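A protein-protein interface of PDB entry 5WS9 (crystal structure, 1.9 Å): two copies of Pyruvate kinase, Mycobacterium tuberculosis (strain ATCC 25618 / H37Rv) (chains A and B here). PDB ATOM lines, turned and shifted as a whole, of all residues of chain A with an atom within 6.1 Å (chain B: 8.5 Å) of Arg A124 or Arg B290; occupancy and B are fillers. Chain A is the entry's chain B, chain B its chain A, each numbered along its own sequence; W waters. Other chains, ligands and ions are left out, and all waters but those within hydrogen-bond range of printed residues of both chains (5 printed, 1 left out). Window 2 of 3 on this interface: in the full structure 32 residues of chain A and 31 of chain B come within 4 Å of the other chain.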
ATOM      1  N   VAL A 120     -20.888 -21.271   2.712  1.00  0.00           N
ATOM      2  CA  VAL A 120     -19.882 -20.576   1.932  1.00  0.00           C
ATOM      3  C   VAL A 120     -18.567 -20.513   2.688  1.00  0.00           C
ATOM      4  O   VAL A 120     -18.542 -20.657   3.905  1.00  0.00           O
ATOM      5  CB  VAL A 120     -20.328 -19.160   1.536  1.00  0.00           C
ATOM      6  CG1 VAL A 120     -21.555 -19.248   0.621  1.00  0.00           C
ATOM      7  CG2 VAL A 120     -20.584 -18.285   2.765  1.00  0.00           C
ATOM      8  N   GLY A 122     -15.645 -19.528   4.864  1.00  0.00           N
ATOM      9  CA  GLY A 122     -15.687 -18.634   6.007  1.00  0.00           C
ATOM     10  C   GLY A 122     -16.759 -18.967   7.050  1.00  0.00           C
ATOM     11  O   GLY A 122     -16.646 -18.559   8.197  1.00  0.00           O
ATOM     12  N   ASP A 123     -17.781 -19.719   6.672  1.00  0.00           N
ATOM     13  CA  ASP A 123     -18.748 -20.189   7.643  1.00  0.00           C
ATOM     14  C   ASP A 123     -18.081 -21.099   8.676  1.00  0.00           C
ATOM     15  O   ASP A 123     -17.167 -21.886   8.370  1.00  0.00           O
ATOM     16  CB  ASP A 123     -19.874 -20.954   6.943  1.00  0.00           C
ATOM     17  CG  ASP A 123     -20.847 -20.021   6.234  1.00  0.00           C
ATOM     18  OD1 ASP A 123     -20.900 -18.847   6.638  1.00  0.00           O
ATOM     19  OD2 ASP A 123     -21.539 -20.443   5.277  1.00  0.00           O
ATOM     20  N   ARG A 124     -18.562 -20.991   9.896  1.00  0.00           N
ATOM     21  CA  ARG A 124     -18.131 -21.838  10.980  1.00  0.00           C
ATOM     22  C   ARG A 124     -19.070 -23.034  11.145  1.00  0.00           C
ATOM     23  O   ARG A 124     -20.292 -22.941  10.945  1.00  0.00           O
ATOM     24  CB  ARG A 124     -18.020 -21.029  12.274  1.00  0.00           C
ATOM     25  CG  ARG A 124     -16.732 -20.218  12.324  1.00  0.00           C
ATOM     26  CD  ARG A 124     -16.717 -19.263  13.499  1.00  0.00           C
ATOM     27  NE  ARG A 124     -16.578 -19.941  14.799  1.00  0.00           N
ATOM     28  CZ  ARG A 124     -15.421 -20.356  15.330  1.00  0.00           C
ATOM     29  NH1 ARG A 124     -14.282 -20.218  14.657  1.00  0.00           N
ATOM     30  NH2 ARG A 124     -15.402 -20.934  16.529  1.00  0.00           N
ATOM     31  N   VAL A 125     -18.473 -24.188  11.426  1.00  0.00           N
ATOM     32  CA  VAL A 125     -19.217 -25.389  11.804  1.00  0.00           C
ATOM     33  C   VAL A 125     -18.782 -25.774  13.206  1.00  0.00           C
ATOM     34  O   VAL A 125     -17.610 -25.982  13.425  1.00  0.00           O
ATOM     35  CB  VAL A 125     -18.913 -26.550  10.866  1.00  0.00           C
ATOM     36  CG1 VAL A 125     -19.830 -27.722  11.201  1.00  0.00           C
ATOM     37  CG2 VAL A 125     -19.128 -26.129   9.442  1.00  0.00           C
ATOM     38  N   LEU A 126     -19.712 -25.785  14.169  1.00  0.00           N
ATOM     39  CA  LEU A 126     -19.402 -26.178  15.533  1.00  0.00           C
ATOM     40  C   LEU A 126     -20.034 -27.536  15.810  1.00  0.00           C
ATOM     41  O   LEU A 126     -21.231 -27.704  15.623  1.00  0.00           O
ATOM     42  CB  LEU A 126     -19.928 -25.127  16.506  1.00  0.00           C
ATOM     43  CG  LEU A 126     -19.399 -23.764  16.055  1.00  0.00           C
ATOM     44  CD1 LEU A 126     -20.204 -22.618  16.566  1.00  0.00           C
ATOM     45  CD2 LEU A 126     -17.903 -23.662  16.355  1.00  0.00           C
ATOM     46  N   ASP A 129     -22.161 -28.797  20.077  1.00  0.00           N
ATOM     47  CA  ASP A 129     -22.189 -27.395  20.524  1.00  0.00           C
ATOM     48  C   ASP A 129     -20.869 -26.777  21.022  1.00  0.00           C
ATOM     49  O   ASP A 129     -20.841 -26.041  22.005  1.00  0.00           O
ATOM     50  CB  ASP A 129     -23.398 -27.116  21.435  1.00  0.00           C
ATOM     51  CG  ASP A 129     -23.310 -27.798  22.765  1.00  0.00           C
ATOM     52  OD1 ASP A 129     -22.937 -27.114  23.745  1.00  0.00           O
ATOM     53  OD2 ASP A 129     -23.644 -29.004  22.837  1.00  0.00           O
ATOM     54  N   GLY A 130     -19.791 -27.060  20.280  1.00  0.00           N
ATOM     55  CA  GLY A 130     -18.527 -26.285  20.349  1.00  0.00           C
ATOM     56  C   GLY A 130     -17.323 -26.887  21.084  1.00  0.00           C
ATOM     57  O   GLY A 130     -16.549 -26.157  21.681  1.00  0.00           O
ATOM     58  N   ALA A 133     -14.411 -27.206  16.378  1.00  0.00           N
ATOM     59  CA  ALA A 133     -14.817 -26.086  15.528  1.00  0.00           C
ATOM     60  C   ALA A 133     -14.092 -26.154  14.182  1.00  0.00           C
ATOM     61  O   ALA A 133     -12.908 -26.493  14.130  1.00  0.00           O
ATOM     62  CB  ALA A 133     -14.588 -24.760  16.214  1.00  0.00           C
ATOM     63  N   LEU A 134     -14.832 -25.982  13.097  1.00  0.00           N
ATOM     64  CA  LEU A 134     -14.260 -26.033  11.742  1.00  0.00           C
ATOM     65  C   LEU A 134     -14.591 -24.746  11.017  1.00  0.00           C
ATOM     66  O   LEU A 134     -15.578 -24.077  11.350  1.00  0.00           O
ATOM     67  CB  LEU A 134     -14.829 -27.201  10.925  1.00  0.00           C
ATOM     68  CG  LEU A 134     -14.778 -28.519  11.720  1.00  0.00           C
ATOM     69  CD1 LEU A 134     -16.152 -29.023  12.084  1.00  0.00           C
ATOM     70  CD2 LEU A 134     -14.030 -29.523  10.944  1.00  0.00           C
ATOM     71  N   VAL A 135     -13.812 -24.446   9.969  1.00  0.00           N
ATOM     72  CA  VAL A 135     -14.126 -23.351   9.101  1.00  0.00           C
ATOM     73  C   VAL A 135     -14.207 -23.866   7.660  1.00  0.00           C
ATOM     74  O   VAL A 135     -13.337 -24.594   7.202  1.00  0.00           O
ATOM     75  CB  VAL A 135     -13.101 -22.201   9.246  1.00  0.00           C
ATOM     76  CG1 VAL A 135     -13.382 -21.112   8.201  1.00  0.00           C
ATOM     77  CG2 VAL A 135     -13.183 -21.601  10.638  1.00  0.00           C
ATOM     78  N   VAL A 136     -15.245 -23.467   6.947  1.00  0.00           N
ATOM     79  CA  VAL A 136     -15.438 -23.920   5.577  1.00  0.00           C
ATOM     80  C   VAL A 136     -14.422 -23.208   4.660  1.00  0.00           C
ATOM     81  O   VAL A 136     -14.253 -21.964   4.737  1.00  0.00           O
ATOM     82  CB  VAL A 136     -16.853 -23.600   5.093  1.00  0.00           C
ATOM     83  CG1 VAL A 136     -17.050 -24.019   3.631  1.00  0.00           C
ATOM     84  CG2 VAL A 136     -17.893 -24.281   5.992  1.00  0.00           C
ATOM     85  N   VAL A 149     -10.271 -25.989  13.152  1.00  0.00           N
ATOM     86  CA  VAL A 149      -9.564 -24.953  13.897  1.00  0.00           C
ATOM     87  C   VAL A 149      -9.502 -25.190  15.394  1.00  0.00           C
ATOM     88  O   VAL A 149      -8.720 -24.570  16.079  1.00  0.00           O
ATOM     89  CB  VAL A 149     -10.059 -23.530  13.593  1.00  0.00           C
ATOM     90  CG1 VAL A 149      -9.890 -23.268  12.107  1.00  0.00           C
ATOM     91  CG2 VAL A 149     -11.514 -23.340  14.015  1.00  0.00           C
ATOM     92  N   GLU A 150     -10.368 -26.063  15.891  1.00  0.00           N
ATOM     93  CA  GLU A 150     -10.312 -26.544  17.268  1.00  0.00           C
ATOM     94  C   GLU A 150     -10.632 -28.006  17.234  1.00  0.00           C
ATOM     95  O   GLU A 150     -11.714 -28.384  16.766  1.00  0.00           O
ATOM     96  CB  GLU A 150     -11.330 -25.814  18.154  1.00  0.00           C
ATOM     97  CG  GLU A 150     -11.099 -24.312  18.246  1.00  0.00           C
ATOM     98  CD  GLU A 150     -11.917 -23.672  19.344  1.00  0.00           C
ATOM     99  OE1 GLU A 150     -12.524 -22.621  19.079  1.00  0.00           O
ATOM    100  OE2 GLU A 150     -11.939 -24.239  20.464  1.00  0.00           O
ATOM    101  N   SER A 161     -23.802 -27.260  14.625  1.00  0.00           N
ATOM    102  CA  SER A 161     -24.436 -25.980  14.501  1.00  0.00           C
ATOM    103  C   SER A 161     -23.722 -25.171  13.425  1.00  0.00           C
ATOM    104  O   SER A 161     -22.507 -25.240  13.279  1.00  0.00           O
ATOM    105  CB  SER A 161     -24.373 -25.230  15.815  1.00  0.00           C
ATOM    106  OG  SER A 161     -24.809 -26.048  16.898  1.00  0.00           O
ATOM    107  N   LEU A 162     -24.496 -24.385  12.696  1.00  0.00           N
ATOM    108  CA  LEU A 162     -24.004 -23.542  11.654  1.00  0.00           C
ATOM    109  C   LEU A 162     -24.361 -22.089  12.033  1.00  0.00           C
ATOM    110  O   LEU A 162     -25.295 -21.495  11.485  1.00  0.00           O
ATOM    111  CB  LEU A 162     -24.659 -23.956  10.334  1.00  0.00           C
ATOM    112  CG  LEU A 162     -24.538 -25.493  10.129  1.00  0.00           C
ATOM    113  CD1 LEU A 162     -25.464 -26.009   9.055  1.00  0.00           C
ATOM    114  CD2 LEU A 162     -23.092 -25.872   9.851  1.00  0.00           C
ATOM    115  N   PRO A 163     -23.633 -21.519  12.991  1.00  0.00           N
ATOM    116  CA  PRO A 163     -24.044 -20.240  13.497  1.00  0.00           C
ATOM    117  C   PRO A 163     -23.937 -19.177  12.415  1.00  0.00           C
ATOM    118  O   PRO A 163     -22.962 -19.154  11.682  1.00  0.00           O
ATOM    119  CB  PRO A 163     -23.055 -19.958  14.624  1.00  0.00           C
ATOM    120  CG  PRO A 163     -21.900 -20.817  14.354  1.00  0.00           C
ATOM    121  CD  PRO A 163     -22.407 -22.003  13.633  1.00  0.00           C
ATOM    122  N   MET A 165     -25.772 -19.110   9.743  1.00  0.00           N
ATOM    123  CA  MET A 165     -26.324 -19.599   8.516  1.00  0.00           C
ATOM    124  C   MET A 165     -27.836 -19.676   8.617  1.00  0.00           C
ATOM    125  O   MET A 165     -28.388 -20.078   9.642  1.00  0.00           O
ATOM    126  CB  MET A 165     -25.730 -20.942   8.156  1.00  0.00           C
ATOM    127  CG  MET A 165     -26.407 -21.621   6.976  1.00  0.00           C
ATOM    128  SD  MET A 165     -25.581 -23.143   6.483  1.00  0.00           S
ATOM    129  CE  MET A 165     -23.863 -22.637   6.670  1.00  0.00           C
ATOM    130  N   GLY A 249     -26.477 -20.232  23.035  1.00  0.00           N
ATOM    131  CA  GLY A 249     -25.121 -19.699  23.152  1.00  0.00           C
ATOM    132  C   GLY A 249     -24.127 -20.199  22.113  1.00  0.00           C
ATOM    133  O   GLY A 249     -22.937 -19.824  22.139  1.00  0.00           O
ATOM    134  N   VAL A 250     -24.600 -21.024  21.187  1.00  0.00           N
ATOM    135  CA  VAL A 250     -23.847 -21.329  20.001  1.00  0.00           C
ATOM    136  C   VAL A 250     -24.447 -20.607  18.805  1.00  0.00           C
ATOM    137  O   VAL A 250     -23.735 -20.114  17.946  1.00  0.00           O
ATOM    138  CB  VAL A 250     -23.851 -22.849  19.775  1.00  0.00           C
ATOM    139  CG1 VAL A 250     -23.421 -23.177  18.354  1.00  0.00           C
ATOM    140  CG2 VAL A 250     -22.931 -23.509  20.804  1.00  0.00           C
ATOM    141  N   LEU A 254     -22.099 -16.228  22.781  1.00  0.00           N
ATOM    142  CA  LEU A 254     -22.410 -16.684  24.124  1.00  0.00           C
ATOM    143  C   LEU A 254     -22.513 -15.532  25.095  1.00  0.00           C
ATOM    144  O   LEU A 254     -23.247 -15.601  26.057  1.00  0.00           O
ATOM    145  CB  LEU A 254     -21.407 -17.724  24.589  1.00  0.00           C
ATOM    146  CG  LEU A 254     -19.948 -17.329  24.764  1.00  0.00           C
ATOM    147  CD1 LEU A 254     -19.745 -16.755  26.146  1.00  0.00           C
ATOM    148  CD2 LEU A 254     -19.039 -18.548  24.568  1.00  0.00           C
ATOM    149  N   LEU B 282     -15.004 -18.434  35.397  1.00  0.00           N
ATOM    150  CA  LEU B 282     -14.971 -19.107  34.102  1.00  0.00           C
ATOM    151  C   LEU B 282     -14.259 -20.441  34.257  1.00  0.00           C
ATOM    152  O   LEU B 282     -13.461 -20.844  33.379  1.00  0.00           O
ATOM    153  CB  LEU B 282     -14.217 -18.206  33.073  1.00  0.00           C
ATOM    154  CG  LEU B 282     -14.902 -16.899  32.634  1.00  0.00           C
ATOM    155  CD1 LEU B 282     -14.085 -16.059  31.657  1.00  0.00           C
ATOM    156  CD2 LEU B 282     -16.283 -17.146  32.031  1.00  0.00           C
ATOM    157  N   ASP B 283     -14.516 -21.099  35.390  1.00  0.00           N
ATOM    158  CA  ASP B 283     -13.741 -22.282  35.830  1.00  0.00           C
ATOM    159  C   ASP B 283     -13.500 -23.315  34.704  1.00  0.00           C
ATOM    160  O   ASP B 283     -12.410 -23.860  34.594  1.00  0.00           O
ATOM    161  CB  ASP B 283     -14.472 -22.984  37.019  1.00  0.00           C
ATOM    162  CG  ASP B 283     -13.646 -24.093  37.640  1.00  0.00           C
ATOM    163  OD1 ASP B 283     -12.678 -23.765  38.275  1.00  0.00           O
ATOM    164  OD2 ASP B 283     -13.942 -25.303  37.452  1.00  0.00           O
ATOM    165  N   SER B 284     -14.530 -23.646  33.945  1.00  0.00           N
ATOM    166  CA  SER B 284     -14.415 -24.722  32.937  1.00  0.00           C
ATOM    167  C   SER B 284     -13.389 -24.368  31.843  1.00  0.00           C
ATOM    168  O   SER B 284     -12.940 -25.242  31.086  1.00  0.00           O
ATOM    169  CB  SER B 284     -15.773 -25.023  32.305  1.00  0.00           C
ATOM    170  OG  SER B 284     -16.199 -23.951  31.478  1.00  0.00           O
ATOM    171  N   MET B 285     -13.060 -23.107  31.707  1.00  0.00           N
ATOM    172  CA  MET B 285     -12.026 -22.683  30.745  1.00  0.00           C
ATOM    173  C   MET B 285     -10.605 -23.060  31.146  1.00  0.00           C
ATOM    174  O   MET B 285      -9.665 -22.870  30.357  1.00  0.00           O
ATOM    175  CB  MET B 285     -12.103 -21.181  30.448  1.00  0.00           C
ATOM    176  CG  MET B 285     -13.356 -20.801  29.673  1.00  0.00           C
ATOM    177  SD  MET B 285     -13.401 -19.146  28.931  1.00  0.00           S
ATOM    178  CE  MET B 285     -12.149 -19.369  27.659  1.00  0.00           C
ATOM    179  N   ILE B 286     -10.439 -23.639  32.343  1.00  0.00           N
ATOM    180  CA  ILE B 286      -9.195 -24.326  32.661  1.00  0.00           C
ATOM    181  C   ILE B 286      -8.906 -25.439  31.644  1.00  0.00           C
ATOM    182  O   ILE B 286      -7.740 -25.641  31.262  1.00  0.00           O
ATOM    183  CB  ILE B 286      -9.178 -24.863  34.118  1.00  0.00           C
ATOM    184  CG1 ILE B 286      -9.047 -23.688  35.074  1.00  0.00           C
ATOM    185  CG2 ILE B 286      -8.019 -25.850  34.315  1.00  0.00           C
ATOM    186  CD1 ILE B 286      -9.458 -23.969  36.498  1.00  0.00           C
ATOM    187  N   GLU B 287      -9.959 -26.132  31.185  1.00  0.00           N
ATOM    188  CA  GLU B 287      -9.805 -27.197  30.190  1.00  0.00           C
ATOM    189  C   GLU B 287     -10.440 -26.907  28.815  1.00  0.00           C
ATOM    190  O   GLU B 287     -10.102 -27.570  27.839  1.00  0.00           O
ATOM    191  CB  GLU B 287     -10.406 -28.501  30.714  1.00  0.00           C
ATOM    192  CG  GLU B 287      -9.810 -28.985  32.010  1.00  0.00           C
ATOM    193  CD  GLU B 287     -10.211 -30.407  32.317  1.00  0.00           C
ATOM    194  OE1 GLU B 287     -10.199 -31.256  31.391  1.00  0.00           O
ATOM    195  OE2 GLU B 287     -10.518 -30.686  33.486  1.00  0.00           O
ATOM    196  N   ASN B 288     -11.388 -25.972  28.751  1.00  0.00           N
ATOM    197  CA  ASN B 288     -12.234 -25.816  27.543  1.00  0.00           C
ATOM    198  C   ASN B 288     -12.077 -24.418  26.970  1.00  0.00           C
ATOM    199  O   ASN B 288     -11.945 -23.439  27.741  1.00  0.00           O
ATOM    200  CB  ASN B 288     -13.714 -26.030  27.909  1.00  0.00           C
ATOM    201  CG  ASN B 288     -13.995 -27.429  28.440  1.00  0.00           C
ATOM    202  OD1 ASN B 288     -13.385 -28.376  28.039  1.00  0.00           O
ATOM    203  ND2 ASN B 288     -15.043 -27.549  29.224  1.00  0.00           N
ATOM    204  N   SER B 289     -12.177 -24.316  25.644  1.00  0.00           N
ATOM    205  CA  SER B 289     -11.972 -23.054  24.921  1.00  0.00           C
ATOM    206  C   SER B 289     -13.142 -22.067  25.076  1.00  0.00           C
ATOM    207  O   SER B 289     -13.004 -20.882  24.786  1.00  0.00           O
ATOM    208  CB  SER B 289     -11.768 -23.327  23.443  1.00  0.00           C
ATOM    209  OG  SER B 289     -12.932 -23.904  22.895  1.00  0.00           O
ATOM    210  N   ARG B 290     -14.290 -22.577  25.493  1.00  0.00           N
ATOM    211  CA  ARG B 290     -15.470 -21.765  25.724  1.00  0.00           C
ATOM    212  C   ARG B 290     -16.053 -22.161  27.075  1.00  0.00           C
ATOM    213  O   ARG B 290     -15.994 -23.351  27.460  1.00  0.00           O
ATOM    214  CB  ARG B 290     -16.520 -22.023  24.629  1.00  0.00           C
ATOM    215  CG  ARG B 290     -16.098 -21.618  23.228  1.00  0.00           C
ATOM    216  CD  ARG B 290     -17.103 -22.139  22.187  1.00  0.00           C
ATOM    217  NE  ARG B 290     -16.912 -21.517  20.880  1.00  0.00           N
ATOM    218  CZ  ARG B 290     -17.842 -21.441  19.936  1.00  0.00           C
ATOM    219  NH1 ARG B 290     -19.069 -21.956  20.138  1.00  0.00           N
ATOM    220  NH2 ARG B 290     -17.551 -20.858  18.785  1.00  0.00           N
ATOM    221  N   PRO B 291     -16.635 -21.189  27.794  1.00  0.00           N
ATOM    222  CA  PRO B 291     -17.164 -21.426  29.134  1.00  0.00           C
ATOM    223  C   PRO B 291     -18.576 -22.093  29.101  1.00  0.00           C
ATOM    224  O   PRO B 291     -19.206 -22.203  28.031  1.00  0.00           O
ATOM    225  CB  PRO B 291     -17.252 -20.015  29.708  1.00  0.00           C
ATOM    226  CG  PRO B 291     -17.612 -19.174  28.521  1.00  0.00           C
ATOM    227  CD  PRO B 291     -16.846 -19.788  27.368  1.00  0.00           C
ATOM    228  N   THR B 292     -19.070 -22.490  30.259  1.00  0.00           N
ATOM    229  CA  THR B 292     -20.450 -22.937  30.371  1.00  0.00           C
ATOM    230  C   THR B 292     -21.419 -21.726  30.403  1.00  0.00           C
ATOM    231  O   THR B 292     -21.017 -20.583  30.554  1.00  0.00           O
ATOM    232  CB  THR B 292     -20.688 -23.762  31.657  1.00  0.00           C
ATOM    233  OG1 THR B 292     -20.639 -22.884  32.799  1.00  0.00           O
ATOM    234  CG2 THR B 292     -19.664 -24.904  31.796  1.00  0.00           C
ATOM    235  N   ARG B 293     -22.691 -22.006  30.242  1.00  0.00           N
ATOM    236  CA  ARG B 293     -23.693 -20.952  30.263  1.00  0.00           C
ATOM    237  C   ARG B 293     -23.821 -20.359  31.694  1.00  0.00           C
ATOM    238  O   ARG B 293     -24.152 -19.176  31.884  1.00  0.00           O
ATOM    239  CB  ARG B 293     -25.024 -21.538  29.788  1.00  0.00           C
ATOM    240  CG  ARG B 293     -24.933 -22.173  28.398  1.00  0.00           C
ATOM    241  CD  ARG B 293     -24.609 -21.149  27.327  1.00  0.00           C
ATOM    242  NE  ARG B 293     -24.426 -21.820  26.047  1.00  0.00           N
ATOM    243  CZ  ARG B 293     -23.274 -22.253  25.564  1.00  0.00           C
ATOM    244  NH1 ARG B 293     -22.143 -22.002  26.205  1.00  0.00           N
ATOM    245  NH2 ARG B 293     -23.243 -22.943  24.418  1.00  0.00           N
ATOM    246  N   GLU B 295     -21.342 -19.962  33.639  1.00  0.00           N
ATOM    247  CA  GLU B 295     -20.177 -19.130  33.799  1.00  0.00           C
ATOM    248  C   GLU B 295     -20.360 -17.749  33.147  1.00  0.00           C
ATOM    249  O   GLU B 295     -20.027 -16.732  33.741  1.00  0.00           O
ATOM    250  CB  GLU B 295     -18.947 -19.873  33.317  1.00  0.00           C
ATOM    251  CG  GLU B 295     -18.464 -20.876  34.341  1.00  0.00           C
ATOM    252  CD  GLU B 295     -17.579 -22.011  33.754  1.00  0.00           C
ATOM    253  OE1 GLU B 295     -17.328 -22.043  32.517  1.00  0.00           O
ATOM    254  OE2 GLU B 295     -17.251 -22.970  34.528  1.00  0.00           O
ATOM    255  N   ALA B 296     -20.895 -17.718  31.943  1.00  0.00           N
ATOM    256  CA  ALA B 296     -21.192 -16.459  31.305  1.00  0.00           C
ATOM    257  C   ALA B 296     -22.213 -15.669  32.139  1.00  0.00           C
ATOM    258  O   ALA B 296     -22.136 -14.452  32.247  1.00  0.00           O
ATOM    259  CB  ALA B 296     -21.728 -16.683  29.911  1.00  0.00           C
ATOM    260  N   TYR B 321      -6.096 -22.240  28.520  1.00  0.00           N
ATOM    261  CA  TYR B 321      -6.578 -21.130  27.705  1.00  0.00           C
ATOM    262  C   TYR B 321      -6.537 -19.779  28.405  1.00  0.00           C
ATOM    263  O   TYR B 321      -7.526 -19.091  28.430  1.00  0.00           O
ATOM    264  CB  TYR B 321      -8.019 -21.403  27.266  1.00  0.00           C
ATOM    265  CG  TYR B 321      -8.163 -22.591  26.385  1.00  0.00           C
ATOM    266  CD1 TYR B 321      -7.891 -22.504  25.033  1.00  0.00           C
ATOM    267  CD2 TYR B 321      -8.565 -23.822  26.907  1.00  0.00           C
ATOM    268  CE1 TYR B 321      -8.021 -23.619  24.213  1.00  0.00           C
ATOM    269  CE2 TYR B 321      -8.694 -24.931  26.109  1.00  0.00           C
ATOM    270  CZ  TYR B 321      -8.431 -24.826  24.757  1.00  0.00           C
ATOM    271  OH  TYR B 321      -8.535 -25.921  23.949  1.00  0.00           O
ATOM    272  N   ALA B 324      -7.557 -16.782  26.089  1.00  0.00           N
ATOM    273  CA  ALA B 324      -8.977 -16.880  25.735  1.00  0.00           C
ATOM    274  C   ALA B 324      -9.866 -16.584  26.921  1.00  0.00           C
ATOM    275  O   ALA B 324     -10.958 -16.001  26.760  1.00  0.00           O
ATOM    276  CB  ALA B 324      -9.295 -18.236  25.141  1.00  0.00           C
ATOM    277  N   ALA B 325      -9.432 -16.974  28.123  1.00  0.00           N
ATOM    278  CA  ALA B 325     -10.222 -16.651  29.320  1.00  0.00           C
ATOM    279  C   ALA B 325     -10.366 -15.146  29.480  1.00  0.00           C
ATOM    280  O   ALA B 325     -11.467 -14.639  29.771  1.00  0.00           O
ATOM    281  CB  ALA B 325      -9.611 -17.284  30.568  1.00  0.00           C
ATOM    282  N   THR B 328     -12.574 -13.681  26.708  1.00  0.00           N
ATOM    283  CA  THR B 328     -13.947 -14.100  26.879  1.00  0.00           C
ATOM    284  C   THR B 328     -14.620 -13.305  27.996  1.00  0.00           C
ATOM    285  O   THR B 328     -15.749 -12.814  27.814  1.00  0.00           O
ATOM    286  CB  THR B 328     -14.051 -15.620  27.129  1.00  0.00           C
ATOM    287  OG1 THR B 328     -13.521 -16.313  25.977  1.00  0.00           O
ATOM    288  CG2 THR B 328     -15.504 -16.036  27.335  1.00  0.00           C
ATOM    289  N   ARG B 331     -15.290  -9.841  26.659  1.00  0.00           N
ATOM    290  CA  ARG B 331     -16.458  -9.796  25.777  1.00  0.00           C
ATOM    291  C   ARG B 331     -17.805  -9.814  26.559  1.00  0.00           C
ATOM    292  O   ARG B 331     -18.756  -9.113  26.186  1.00  0.00           O
ATOM    293  CB  ARG B 331     -16.430 -10.916  24.738  1.00  0.00           C
ATOM    294  CG  ARG B 331     -15.425 -10.702  23.647  1.00  0.00           C
ATOM    295  CD  ARG B 331     -15.636 -11.659  22.489  1.00  0.00           C
ATOM    296  NE  ARG B 331     -15.444 -13.041  22.889  1.00  0.00           N
ATOM    297  CZ  ARG B 331     -14.292 -13.723  22.815  1.00  0.00           C
ATOM    298  NH1 ARG B 331     -13.177 -13.187  22.341  1.00  0.00           N
ATOM    299  NH2 ARG B 331     -14.271 -14.980  23.197  1.00  0.00           N
HETATM  300  O   HOH W   1     -18.868 -19.303  16.186  1.00  0.00           O
HETATM  301  O   HOH W   2      -9.025 -25.676  21.336  1.00  0.00           O
HETATM  302  O   HOH W   3     -12.017 -26.903  21.496  1.00  0.00           O
HETATM  303  O   HOH W   4     -21.894 -25.160  26.026  1.00  0.00           O
HETATM  304  O   HOH W   5     -15.257 -25.451  24.119  1.00  0.00           O
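The side-chain carboxylate of Glu A150 is in hydrogen-bond range of the side-chain hydroxyl of Ser B289 (2.6 Å).
The guanidinium group (NH2) of Arg A124 lies close to the guanidinium group (NH2) of Arg B290 (3.1 Å).
Water W2 bridges OH of Tyr B321 and OE2 of Glu A150.
Water W1 bridges NE of Arg A124 (2.8 Å) and NH2 of Arg B290 (3.3 Å).
Water W5 lies within hydrogen-bond range of the backbone carbonyl oxygen of Gly A130 (2.8 Å), the side-chain hydroxyl of Ser B289 (3.0 Å) and the backbone NH of Arg B290 (3.3 Å).
Water W3 lies within hydrogen-bond range of OE2 of Glu A150 (2.9 Å) and OG of Ser B289 (3.4 Å).
Water W4 lies within hydrogen-bond range of the guanidinium group (NH2) of Arg B293 (3.1 Å) and the side-chain carboxylate (OD1) of Asp A129 (3.2 Å).
Among the printed residues, pairs that only touch across the chains: Leu A126 with Arg B290, Gly A249 with Arg B293, Val A250 with Arg B293 and Leu A254 with Pro B291.
No position is printed for both chains.
Of the 6 pairs that touch across the chains among the printed residues, none has its exchanged pair printed and touching as well.
Of the 21 printed residues of chain A, 6 touch a printed residue of chain B.
Printed residues of chain A that touch a printed residue of chain B: Arg A124, Leu A126, Glu A150, Gly A249, Val A250 and Leu A254.
Hydrophobic or aromatic side chains of chain A that line the printed part of chain B: Leu A126, Val A250 and Leu A254.
Hydrophobic or aromatic side chains of chain B that line the printed part of chain A: Pro B291.
Among the printed residues, no Asp or Glu carboxylate lies within 4 Å of a Lys or Arg side-chain nitrogen of the other chain.
Of the printed residues of chain B, Arg A124 touches Arg B290.
Of the printed residues of chain A, Arg B290 touches Arg A124 (3.1 Å) and Leu A126 (3.7 Å).
Of the printed residues of chain A, Arg B293 touches Gly A249 and Val A250.
Printed residues of chain B within 4 Å of Leu A126: Arg B290.
Ile B286 touches none of the printed residues of chain A.
Ser B284 touches none of the printed residues of chain A.
The nearest printed residue of chain A that does not touch Arg B290 is Gly A130 (4.1 Å).
NH1 of Arg B293 sits at hydrogen-bond distance from O of Pro B291 (3.5 Å).
O of Leu A126 lies within hydrogen-bond range of N of Ser A161 (2.8 Å).
The backbone NH of Ala A133 sits at hydrogen-bond distance from the backbone carbonyl oxygen of Glu A150 (3.0 Å).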
